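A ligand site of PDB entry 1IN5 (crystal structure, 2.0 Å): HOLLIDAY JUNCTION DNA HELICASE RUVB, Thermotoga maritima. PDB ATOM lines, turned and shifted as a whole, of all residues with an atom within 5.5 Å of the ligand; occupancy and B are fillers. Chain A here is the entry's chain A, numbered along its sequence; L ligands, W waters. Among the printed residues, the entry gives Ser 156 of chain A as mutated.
Gln 17 touches the ligand. Leu 19 touches the ligand. CA of Arg 20 touches O10 of the ligand, at 3.0 Å. CG of Pro 21 touches C9 of the ligand (3.6 Å). Phe 27 touches the ligand. Pro 60 touches the ligand. CG2 of Ile 188 touches C9 of the ligand (3.8 Å). Pro 216 touches the ligand. Arg 217 touches the ligand (CB to C1, 3.7 Å). CD1 of Ile 220 touches C5 of the ligand (3.6 Å). Hydrophobic or aromatic side chains within 4 Å of the ligand: Pro 21, Phe 27, Tyr 180, Ile 188, Pro 216 and Ile 220. Within 4 Å of the ligand: Gln 17, Leu 19, Arg 20, Pro 21, Phe 27, Ile 28, Pro 60, Gly 61, Leu 62, Gly 63, Lys 64, Thr 65, Thr 66, Tyr 180, Ile 188, Pro 216, Arg 217 and Ile 220.
Water W5 lies within hydrogen-bond range of N4 of the ligand, O of Glu 26 and N of Ile 28. Water W1 bridges an oxygen (O5) of the ligand and the guanidinium group (NH2) of Arg 20. Water W7 lies within hydrogen-bond range of the side-chain hydroxyl of Ser 156 (2.6 Å), the side-chain carboxylate of Asp 109 (2.7 Å), an oxygen (O2) of the ligand (2.7 Å) and the side-chain hydroxyl of Thr 65 (3.5 Å). Water W2 bridges an oxygen (O5) of the ligand (2.8 Å) and the side-chain hydroxyl (OG1) of Thr 65 (3.2 Å). Water W6 lies within hydrogen-bond range of O of Leu 19 (2.7 Å) and N5 of the ligand (2.8 Å). Water W4 bridges an oxygen (O5) of the ligand and the guanidinium group (NE) of Arg 217.
N of Gly 61 lies within hydrogen-bond range of O3 of the ligand. The backbone NH (N) of Thr 66 is in hydrogen-bond range of an oxygen (O4) of the ligand, 2.9 Å away. OG1 of Thr 66 sits at hydrogen-bond distance from O4 of the ligand. The backbone carbonyl oxygen (O) of Ile 28 is in hydrogen-bond range of a nitrogen (N3) of the ligand (2.9 Å). An oxygen (O2) of the ligand lies within hydrogen-bond range of the backbone NH (N) of Thr 65, at 3.0 Å. The side-chain hydroxyl (OG1) of Thr 65 sits at hydrogen-bond distance from an oxygen (O2) of the ligand. N of Lys 64 lies within hydrogen-bond range of O1 of the ligand. The side-chain amino group of Lys 64 lies within salt-bridge range of an oxygen (O1) of the ligand (2.9 Å). The backbone NH of Gly 63 sits at hydrogen-bond distance from an oxygen (O1) of the ligand (3.2 Å). OH of Tyr 180 is in hydrogen-bond range of N3 of the ligand (3.1 Å). An oxygen (O1) of the ligand is in hydrogen-bond range of the backbone NH (N) of Leu 62 (3.2 Å).
O of Gly 61 lies within hydrogen-bond range of N of Arg 217. The backbone carbonyl oxygen (O) of Pro 59 is in hydrogen-bond range of the side-chain amino group (NZ) of Lys 64 (2.8 Å). O of Gly 58 lies within hydrogen-bond range of NZ of Lys 64 (2.7 Å). OE1 of Gln 17 lies within hydrogen-bond range of NH2 of Arg 20, 3.0 Å away. O of Leu 62 is in hydrogen-bond range of OH of Tyr 180 (2.7 Å). The backbone carbonyl oxygen (O) of Leu 19 lies within hydrogen-bond range of the guanidinium group (NH2) of Arg 191, at 2.9 Å.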
ATOM      1  N   GLN A  17     -12.585   2.783  25.341  1.00  0.00           N
ATOM      2  CA  GLN A  17     -12.411   1.317  25.131  1.00  0.00           C
ATOM      3  C   GLN A  17     -11.119   0.851  25.779  1.00  0.00           C
ATOM      4  O   GLN A  17     -10.506  -0.131  25.361  1.00  0.00           O
ATOM      5  CB  GLN A  17     -12.371   1.018  23.624  1.00  0.00           C
ATOM      6  CG  GLN A  17     -12.734  -0.415  23.270  1.00  0.00           C
ATOM      7  CD  GLN A  17     -14.213  -0.709  23.474  1.00  0.00           C
ATOM      8  OE1 GLN A  17     -15.060  -0.141  22.790  1.00  0.00           O
ATOM      9  NE2 GLN A  17     -14.520  -1.578  24.432  1.00  0.00           N
ATOM     10  N   LEU A  19     -10.825  -0.519  28.520  1.00  0.00           N
ATOM     11  CA  LEU A  19     -11.069  -1.699  29.324  1.00  0.00           C
ATOM     12  C   LEU A  19     -11.112  -2.962  28.473  1.00  0.00           C
ATOM     13  O   LEU A  19     -11.082  -4.076  28.997  1.00  0.00           O
ATOM     14  CB  LEU A  19     -12.390  -1.561  30.092  1.00  0.00           C
ATOM     15  CG  LEU A  19     -12.441  -0.497  31.200  1.00  0.00           C
ATOM     16  CD1 LEU A  19     -13.816  -0.480  31.848  1.00  0.00           C
ATOM     17  CD2 LEU A  19     -11.365  -0.794  32.231  1.00  0.00           C
ATOM     18  N   ARG A  20     -11.153  -2.791  27.155  1.00  0.00           N
ATOM     19  CA  ARG A  20     -11.200  -3.921  26.250  1.00  0.00           C
ATOM     20  C   ARG A  20      -9.818  -4.531  25.964  1.00  0.00           C
ATOM     21  O   ARG A  20      -8.880  -3.815  25.634  1.00  0.00           O
ATOM     22  CB  ARG A  20     -11.845  -3.508  24.924  1.00  0.00           C
ATOM     23  CG  ARG A  20     -11.917  -4.656  23.933  1.00  0.00           C
ATOM     24  CD  ARG A  20     -12.144  -4.152  22.527  1.00  0.00           C
ATOM     25  NE  ARG A  20     -13.484  -3.622  22.338  1.00  0.00           N
ATOM     26  CZ  ARG A  20     -13.891  -3.052  21.213  1.00  0.00           C
ATOM     27  NH1 ARG A  20     -13.066  -2.940  20.177  1.00  0.00           N
ATOM     28  NH2 ARG A  20     -15.134  -2.584  21.113  1.00  0.00           N
ATOM     29  N   PRO A  21      -9.699  -5.862  26.082  1.00  0.00           N
ATOM     30  CA  PRO A  21      -8.425  -6.540  25.819  1.00  0.00           C
ATOM     31  C   PRO A  21      -7.948  -6.241  24.400  1.00  0.00           C
ATOM     32  O   PRO A  21      -8.745  -6.239  23.458  1.00  0.00           O
ATOM     33  CB  PRO A  21      -8.780  -8.019  26.005  1.00  0.00           C
ATOM     34  CG  PRO A  21      -9.834  -7.971  27.053  1.00  0.00           C
ATOM     35  CD  PRO A  21     -10.696  -6.817  26.612  1.00  0.00           C
ATOM     36  N   GLU A  26      -4.346 -10.599  27.000  1.00  0.00           N
ATOM     37  CA  GLU A  26      -5.126  -9.750  27.894  1.00  0.00           C
ATOM     38  C   GLU A  26      -6.563 -10.250  28.010  1.00  0.00           C
ATOM     39  O   GLU A  26      -7.362  -9.657  28.737  1.00  0.00           O
ATOM     40  CB  GLU A  26      -5.154  -8.300  27.395  1.00  0.00           C
ATOM     41  CG  GLU A  26      -3.845  -7.560  27.554  1.00  0.00           C
ATOM     42  CD  GLU A  26      -3.889  -6.151  26.997  1.00  0.00           C
ATOM     43  OE1 GLU A  26      -2.797  -5.557  26.829  1.00  0.00           O
ATOM     44  OE2 GLU A  26      -4.994  -5.630  26.711  1.00  0.00           O
ATOM     45  N   PHE A  27      -6.874 -11.330  27.322  1.00  0.00           N
ATOM     46  CA  PHE A  27      -8.233 -11.880  27.321  1.00  0.00           C
ATOM     47  C   PHE A  27      -8.382 -13.013  28.327  1.00  0.00           C
ATOM     48  O   PHE A  27      -7.914 -14.128  28.111  1.00  0.00           O
ATOM     49  CB  PHE A  27      -8.563 -12.374  25.900  1.00  0.00           C
ATOM     50  CG  PHE A  27     -10.035 -12.554  25.635  1.00  0.00           C
ATOM     51  CD1 PHE A  27     -10.700 -13.709  26.050  1.00  0.00           C
ATOM     52  CD2 PHE A  27     -10.754 -11.586  24.929  1.00  0.00           C
ATOM     53  CE1 PHE A  27     -12.046 -13.908  25.745  1.00  0.00           C
ATOM     54  CE2 PHE A  27     -12.099 -11.776  24.621  1.00  0.00           C
ATOM     55  CZ  PHE A  27     -12.756 -12.936  25.026  1.00  0.00           C
ATOM     56  N   ILE A  28      -9.034 -12.714  29.448  1.00  0.00           N
ATOM     57  CA  ILE A  28      -9.256 -13.705  30.505  1.00  0.00           C
ATOM     58  C   ILE A  28     -10.384 -14.669  30.139  1.00  0.00           C
ATOM     59  O   ILE A  28     -11.414 -14.249  29.627  1.00  0.00           O
ATOM     60  CB  ILE A  28      -9.588 -13.006  31.846  1.00  0.00           C
ATOM     61  CG1 ILE A  28      -8.392 -12.179  32.288  1.00  0.00           C
ATOM     62  CG2 ILE A  28      -9.959 -14.055  32.898  1.00  0.00           C
ATOM     63  CD1 ILE A  28      -8.597 -11.448  33.583  1.00  0.00           C
ATOM     64  N   GLY A  29     -10.162 -15.950  30.415  1.00  0.00           N
ATOM     65  CA  GLY A  29     -11.177 -16.946  30.113  1.00  0.00           C
ATOM     66  C   GLY A  29     -11.219 -17.391  28.662  1.00  0.00           C
ATOM     67  O   GLY A  29     -10.422 -16.942  27.838  1.00  0.00           O
ATOM     68  N   GLY A  58     -22.127 -17.213  20.268  1.00  0.00           N
ATOM     69  CA  GLY A  58     -22.385 -17.258  21.698  1.00  0.00           C
ATOM     70  C   GLY A  58     -23.211 -16.073  22.164  1.00  0.00           C
ATOM     71  O   GLY A  58     -23.360 -15.091  21.428  1.00  0.00           O
ATOM     72  N   PRO A  59     -23.765 -16.129  23.376  1.00  0.00           N
ATOM     73  CA  PRO A  59     -24.560 -14.984  23.838  1.00  0.00           C
ATOM     74  C   PRO A  59     -23.799 -13.667  23.843  1.00  0.00           C
ATOM     75  O   PRO A  59     -22.570 -13.649  23.867  1.00  0.00           O
ATOM     76  CB  PRO A  59     -25.040 -15.410  25.236  1.00  0.00           C
ATOM     77  CG  PRO A  59     -24.107 -16.507  25.633  1.00  0.00           C
ATOM     78  CD  PRO A  59     -23.827 -17.230  24.343  1.00  0.00           C
ATOM     79  N   PRO A  60     -24.520 -12.549  23.817  1.00  0.00           N
ATOM     80  CA  PRO A  60     -23.923 -11.222  23.818  1.00  0.00           C
ATOM     81  C   PRO A  60     -23.160 -10.889  25.104  1.00  0.00           C
ATOM     82  O   PRO A  60     -23.465 -11.423  26.172  1.00  0.00           O
ATOM     83  CB  PRO A  60     -25.131 -10.309  23.591  1.00  0.00           C
ATOM     84  CG  PRO A  60     -26.251 -11.058  24.225  1.00  0.00           C
ATOM     85  CD  PRO A  60     -25.997 -12.480  23.801  1.00  0.00           C
ATOM     86  N   GLY A  61     -22.155 -10.035  24.972  1.00  0.00           N
ATOM     87  CA  GLY A  61     -21.365  -9.610  26.113  1.00  0.00           C
ATOM     88  C   GLY A  61     -20.215 -10.530  26.493  1.00  0.00           C
ATOM     89  O   GLY A  61     -19.528 -10.285  27.479  1.00  0.00           O
ATOM     90  N   LEU A  62     -19.990 -11.569  25.686  1.00  0.00           N
ATOM     91  CA  LEU A  62     -18.948 -12.542  25.955  1.00  0.00           C
ATOM     92  C   LEU A  62     -17.600 -12.292  25.307  1.00  0.00           C
ATOM     93  O   LEU A  62     -16.674 -13.067  25.488  1.00  0.00           O
ATOM     94  CB  LEU A  62     -19.420 -13.949  25.581  1.00  0.00           C
ATOM     95  CG  LEU A  62     -20.677 -14.483  26.275  1.00  0.00           C
ATOM     96  CD1 LEU A  62     -20.967 -15.879  25.744  1.00  0.00           C
ATOM     97  CD2 LEU A  62     -20.480 -14.526  27.787  1.00  0.00           C
ATOM     98  N   GLY A  63     -17.486 -11.223  24.512  1.00  0.00           N
ATOM     99  CA  GLY A  63     -16.217 -10.926  23.886  1.00  0.00           C
ATOM    100  C   GLY A  63     -16.002 -11.295  22.433  1.00  0.00           C
ATOM    101  O   GLY A  63     -14.852 -11.392  21.996  1.00  0.00           O
ATOM    102  N   LYS A  64     -17.084 -11.480  21.676  1.00  0.00           N
ATOM    103  CA  LYS A  64     -16.968 -11.846  20.263  1.00  0.00           C
ATOM    104  C   LYS A  64     -16.374 -10.676  19.449  1.00  0.00           C
ATOM    105  O   LYS A  64     -15.476 -10.867  18.630  1.00  0.00           O
ATOM    106  CB  LYS A  64     -18.339 -12.292  19.725  1.00  0.00           C
ATOM    107  CG  LYS A  64     -18.863 -13.603  20.349  1.00  0.00           C
ATOM    108  CD  LYS A  64     -20.152 -14.086  19.701  1.00  0.00           C
ATOM    109  CE  LYS A  64     -21.276 -13.093  19.871  1.00  0.00           C
ATOM    110  NZ  LYS A  64     -21.759 -12.906  21.276  1.00  0.00           N
ATOM    111  N   THR A  65     -16.879  -9.476  19.696  1.00  0.00           N
ATOM    112  CA  THR A  65     -16.370  -8.284  19.009  1.00  0.00           C
ATOM    113  C   THR A  65     -14.895  -8.098  19.378  1.00  0.00           C
ATOM    114  O   THR A  65     -14.042  -7.875  18.535  1.00  0.00           O
ATOM    115  CB  THR A  65     -17.162  -7.018  19.419  1.00  0.00           C
ATOM    116  OG1 THR A  65     -18.506  -7.141  18.970  1.00  0.00           O
ATOM    117  CG2 THR A  65     -16.537  -5.767  18.807  1.00  0.00           C
ATOM    118  N   THR A  66     -14.628  -8.224  20.680  1.00  0.00           N
ATOM    119  CA  THR A  66     -13.283  -8.091  21.211  1.00  0.00           C
ATOM    120  C   THR A  66     -12.319  -9.023  20.483  1.00  0.00           C
ATOM    121  O   THR A  66     -11.214  -8.607  20.083  1.00  0.00           O
ATOM    122  CB  THR A  66     -13.262  -8.420  22.705  1.00  0.00           C
ATOM    123  OG1 THR A  66     -14.136  -7.530  23.399  1.00  0.00           O
ATOM    124  CG2 THR A  66     -11.870  -8.287  23.291  1.00  0.00           C
ATOM    125  N   LEU A  67     -12.720 -10.271  20.309  1.00  0.00           N
ATOM    126  CA  LEU A  67     -11.851 -11.231  19.629  1.00  0.00           C
ATOM    127  C   LEU A  67     -11.643 -10.872  18.166  1.00  0.00           C
ATOM    128  O   LEU A  67     -10.547 -11.061  17.631  1.00  0.00           O
ATOM    129  CB  LEU A  67     -12.437 -12.648  19.742  1.00  0.00           C
ATOM    130  CG  LEU A  67     -12.392 -13.220  21.153  1.00  0.00           C
ATOM    131  CD1 LEU A  67     -13.193 -14.515  21.212  1.00  0.00           C
ATOM    132  CD2 LEU A  67     -10.926 -13.463  21.563  1.00  0.00           C
ATOM    133  N   ASP A 109     -21.235  -8.298  12.482  1.00  0.00           N
ATOM    134  CA  ASP A 109     -22.004  -8.620  13.655  1.00  0.00           C
ATOM    135  C   ASP A 109     -23.392  -9.085  13.202  1.00  0.00           C
ATOM    136  O   ASP A 109     -23.887  -8.659  12.165  1.00  0.00           O
ATOM    137  CB  ASP A 109     -22.127  -7.374  14.543  1.00  0.00           C
ATOM    138  CG  ASP A 109     -22.677  -7.690  15.907  1.00  0.00           C
ATOM    139  OD1 ASP A 109     -22.139  -8.610  16.556  1.00  0.00           O
ATOM    140  OD2 ASP A 109     -23.647  -7.019  16.318  1.00  0.00           O
ATOM    141  N   SER A 156     -20.169 -12.877  13.449  1.00  0.00           N
ATOM    142  CA  SER A 156     -20.555 -13.007  14.846  1.00  0.00           C
ATOM    143  C   SER A 156     -22.041 -13.308  14.915  1.00  0.00           C
ATOM    144  O   SER A 156     -22.845 -12.690  14.216  1.00  0.00           O
ATOM    145  CB  SER A 156     -20.257 -11.716  15.594  1.00  0.00           C
ATOM    146  OG  SER A 156     -20.663 -11.826  16.946  1.00  0.00           O
ATOM    147  N   TYR A 180     -18.897 -17.383  31.268  1.00  0.00           N
ATOM    148  CA  TYR A 180     -17.647 -17.476  32.013  1.00  0.00           C
ATOM    149  C   TYR A 180     -17.887 -17.989  33.426  1.00  0.00           C
ATOM    150  O   TYR A 180     -19.028 -17.961  33.917  1.00  0.00           O
ATOM    151  CB  TYR A 180     -16.976 -16.105  32.113  1.00  0.00           C
ATOM    152  CG  TYR A 180     -16.413 -15.558  30.819  1.00  0.00           C
ATOM    153  CD1 TYR A 180     -17.238 -15.269  29.731  1.00  0.00           C
ATOM    154  CD2 TYR A 180     -15.040 -15.311  30.693  1.00  0.00           C
ATOM    155  CE1 TYR A 180     -16.717 -14.728  28.543  1.00  0.00           C
ATOM    156  CE2 TYR A 180     -14.521 -14.785  29.522  1.00  0.00           C
ATOM    157  CZ  TYR A 180     -15.354 -14.496  28.457  1.00  0.00           C
ATOM    158  OH  TYR A 180     -14.817 -13.953  27.309  1.00  0.00           O
ATOM    159  N   ILE A 188     -11.756 -10.611  35.855  1.00  0.00           N
ATOM    160  CA  ILE A 188     -12.070  -9.565  34.883  1.00  0.00           C
ATOM    161  C   ILE A 188     -12.450  -8.300  35.654  1.00  0.00           C
ATOM    162  O   ILE A 188     -12.072  -7.192  35.278  1.00  0.00           O
ATOM    163  CB  ILE A 188     -13.228 -10.019  33.952  1.00  0.00           C
ATOM    164  CG1 ILE A 188     -12.688 -11.108  33.015  1.00  0.00           C
ATOM    165  CG2 ILE A 188     -13.784  -8.856  33.159  1.00  0.00           C
ATOM    166  CD1 ILE A 188     -13.768 -11.876  32.273  1.00  0.00           C
ATOM    167  N   ARG A 191      -9.399  -6.661  37.199  1.00  0.00           N
ATOM    168  CA  ARG A 191      -8.676  -6.015  36.108  1.00  0.00           C
ATOM    169  C   ARG A 191      -9.341  -4.689  35.742  1.00  0.00           C
ATOM    170  O   ARG A 191      -8.660  -3.686  35.537  1.00  0.00           O
ATOM    171  CB  ARG A 191      -8.654  -6.934  34.881  1.00  0.00           C
ATOM    172  CG  ARG A 191      -8.085  -6.296  33.629  1.00  0.00           C
ATOM    173  CD  ARG A 191      -7.987  -7.317  32.486  1.00  0.00           C
ATOM    174  NE  ARG A 191      -7.442  -6.744  31.251  1.00  0.00           N
ATOM    175  CZ  ARG A 191      -8.072  -5.849  30.488  1.00  0.00           C
ATOM    176  NH1 ARG A 191      -7.489  -5.393  29.393  1.00  0.00           N
ATOM    177  NH2 ARG A 191      -9.277  -5.429  30.826  1.00  0.00           N
ATOM    178  N   PRO A 216     -18.976 -11.020  30.941  1.00  0.00           N
ATOM    179  CA  PRO A 216     -18.004  -9.966  31.199  1.00  0.00           C
ATOM    180  C   PRO A 216     -18.612  -8.554  31.062  1.00  0.00           C
ATOM    181  O   PRO A 216     -18.336  -7.672  31.868  1.00  0.00           O
ATOM    182  CB  PRO A 216     -16.923 -10.246  30.161  1.00  0.00           C
ATOM    183  CG  PRO A 216     -16.969 -11.751  30.016  1.00  0.00           C
ATOM    184  CD  PRO A 216     -18.466 -11.998  29.962  1.00  0.00           C
ATOM    185  N   ARG A 217     -19.439  -8.340  30.032  1.00  0.00           N
ATOM    186  CA  ARG A 217     -20.033  -7.008  29.834  1.00  0.00           C
ATOM    187  C   ARG A 217     -20.868  -6.606  31.040  1.00  0.00           C
ATOM    188  O   ARG A 217     -20.814  -5.456  31.487  1.00  0.00           O
ATOM    189  CB  ARG A 217     -20.916  -7.001  28.574  1.00  0.00           C
ATOM    190  CG  ARG A 217     -21.491  -5.623  28.249  1.00  0.00           C
ATOM    191  CD  ARG A 217     -22.184  -5.646  26.898  1.00  0.00           C
ATOM    192  NE  ARG A 217     -22.599  -4.321  26.463  1.00  0.00           N
ATOM    193  CZ  ARG A 217     -23.709  -3.704  26.855  1.00  0.00           C
ATOM    194  NH1 ARG A 217     -24.525  -4.287  27.717  1.00  0.00           N
ATOM    195  NH2 ARG A 217     -23.991  -2.504  26.393  1.00  0.00           N
ATOM    196  N   ILE A 220     -18.535  -5.834  34.127  1.00  0.00           N
ATOM    197  CA  ILE A 220     -17.853  -4.542  34.027  1.00  0.00           C
ATOM    198  C   ILE A 220     -18.787  -3.367  34.291  1.00  0.00           C
ATOM    199  O   ILE A 220     -18.394  -2.396  34.937  1.00  0.00           O
ATOM    200  CB  ILE A 220     -17.216  -4.362  32.639  1.00  0.00           C
ATOM    201  CG1 ILE A 220     -16.133  -5.424  32.436  1.00  0.00           C
ATOM    202  CG2 ILE A 220     -16.595  -2.973  32.528  1.00  0.00           C
ATOM    203  CD1 ILE A 220     -15.702  -5.587  30.979  1.00  0.00           C
HETATM  204  P1  LIG L   1     -20.005  -9.526  22.286  1.00  0.00           P
HETATM  205  O1  LIG L   1     -19.897 -10.984  22.493  1.00  0.00           O
HETATM  206  O2  LIG L   1     -19.594  -9.044  20.882  1.00  0.00           O
HETATM  207  O3  LIG L   1     -21.442  -9.019  22.586  1.00  0.00           O
HETATM  208  P2  LIG L   1     -17.980  -7.682  23.359  1.00  0.00           P
HETATM  209  O4  LIG L   1     -16.742  -8.158  22.690  1.00  0.00           O
HETATM  210  O5  LIG L   1     -18.546  -6.476  22.758  1.00  0.00           O
HETATM  211  O6  LIG L   1     -19.182  -8.816  23.367  1.00  0.00           O
HETATM  212  O7  LIG L   1     -17.751  -7.438  24.896  1.00  0.00           O
HETATM  213  C1  LIG L   1     -18.306  -6.716  25.951  1.00  0.00           C
HETATM  214  C2  LIG L   1     -17.546  -5.944  26.786  1.00  0.00           C
HETATM  215  O8  LIG L   1     -17.008  -6.872  27.642  1.00  0.00           O
HETATM  216  C3  LIG L   1     -16.238  -5.373  26.187  1.00  0.00           C
HETATM  217  O9  LIG L   1     -16.266  -4.151  26.861  1.00  0.00           O
HETATM  218  C4  LIG L   1     -15.070  -6.016  26.673  1.00  0.00           C
HETATM  219  O10 LIG L   1     -13.972  -5.067  26.609  1.00  0.00           O
HETATM  220  C5  LIG L   1     -15.710  -7.058  27.711  1.00  0.00           C
HETATM  221  N1  LIG L   1     -15.197  -8.333  27.616  1.00  0.00           N
HETATM  222  C6  LIG L   1     -15.616  -9.408  26.882  1.00  0.00           C
HETATM  223  N2  LIG L   1     -14.922 -10.435  27.022  1.00  0.00           N
HETATM  224  C7  LIG L   1     -13.935 -10.055  27.893  1.00  0.00           C
HETATM  225  C8  LIG L   1     -12.774 -10.735  28.480  1.00  0.00           C
HETATM  226  N3  LIG L   1     -12.528 -12.040  28.189  1.00  0.00           N
HETATM  227  N4  LIG L   1     -11.923 -10.035  29.375  1.00  0.00           N
HETATM  228  C9  LIG L   1     -12.192  -8.701  29.672  1.00  0.00           C
HETATM  229  N5  LIG L   1     -13.252  -7.981  29.160  1.00  0.00           N
HETATM  230  C10 LIG L   1     -14.078  -8.707  28.267  1.00  0.00           C
HETATM  231  O   HOH W   1     -17.075  -4.328  22.353  1.00  0.00           O
HETATM  232  O   HOH W   2     -20.572  -5.839  20.990  1.00  0.00           O
HETATM  233  O   HOH W   3     -23.373  -8.881  20.819  1.00  0.00           O
HETATM  234  O   HOH W   4     -21.145  -4.821  23.472  1.00  0.00           O
HETATM  235  O   HOH W   5      -9.522 -10.006  30.317  1.00  0.00           O
HETATM  236  O   HOH W   6     -12.809  -5.570  30.497  1.00  0.00           O
HETATM  237  O   HOH W   7     -20.779  -9.747  18.570  1.00  0.00           O
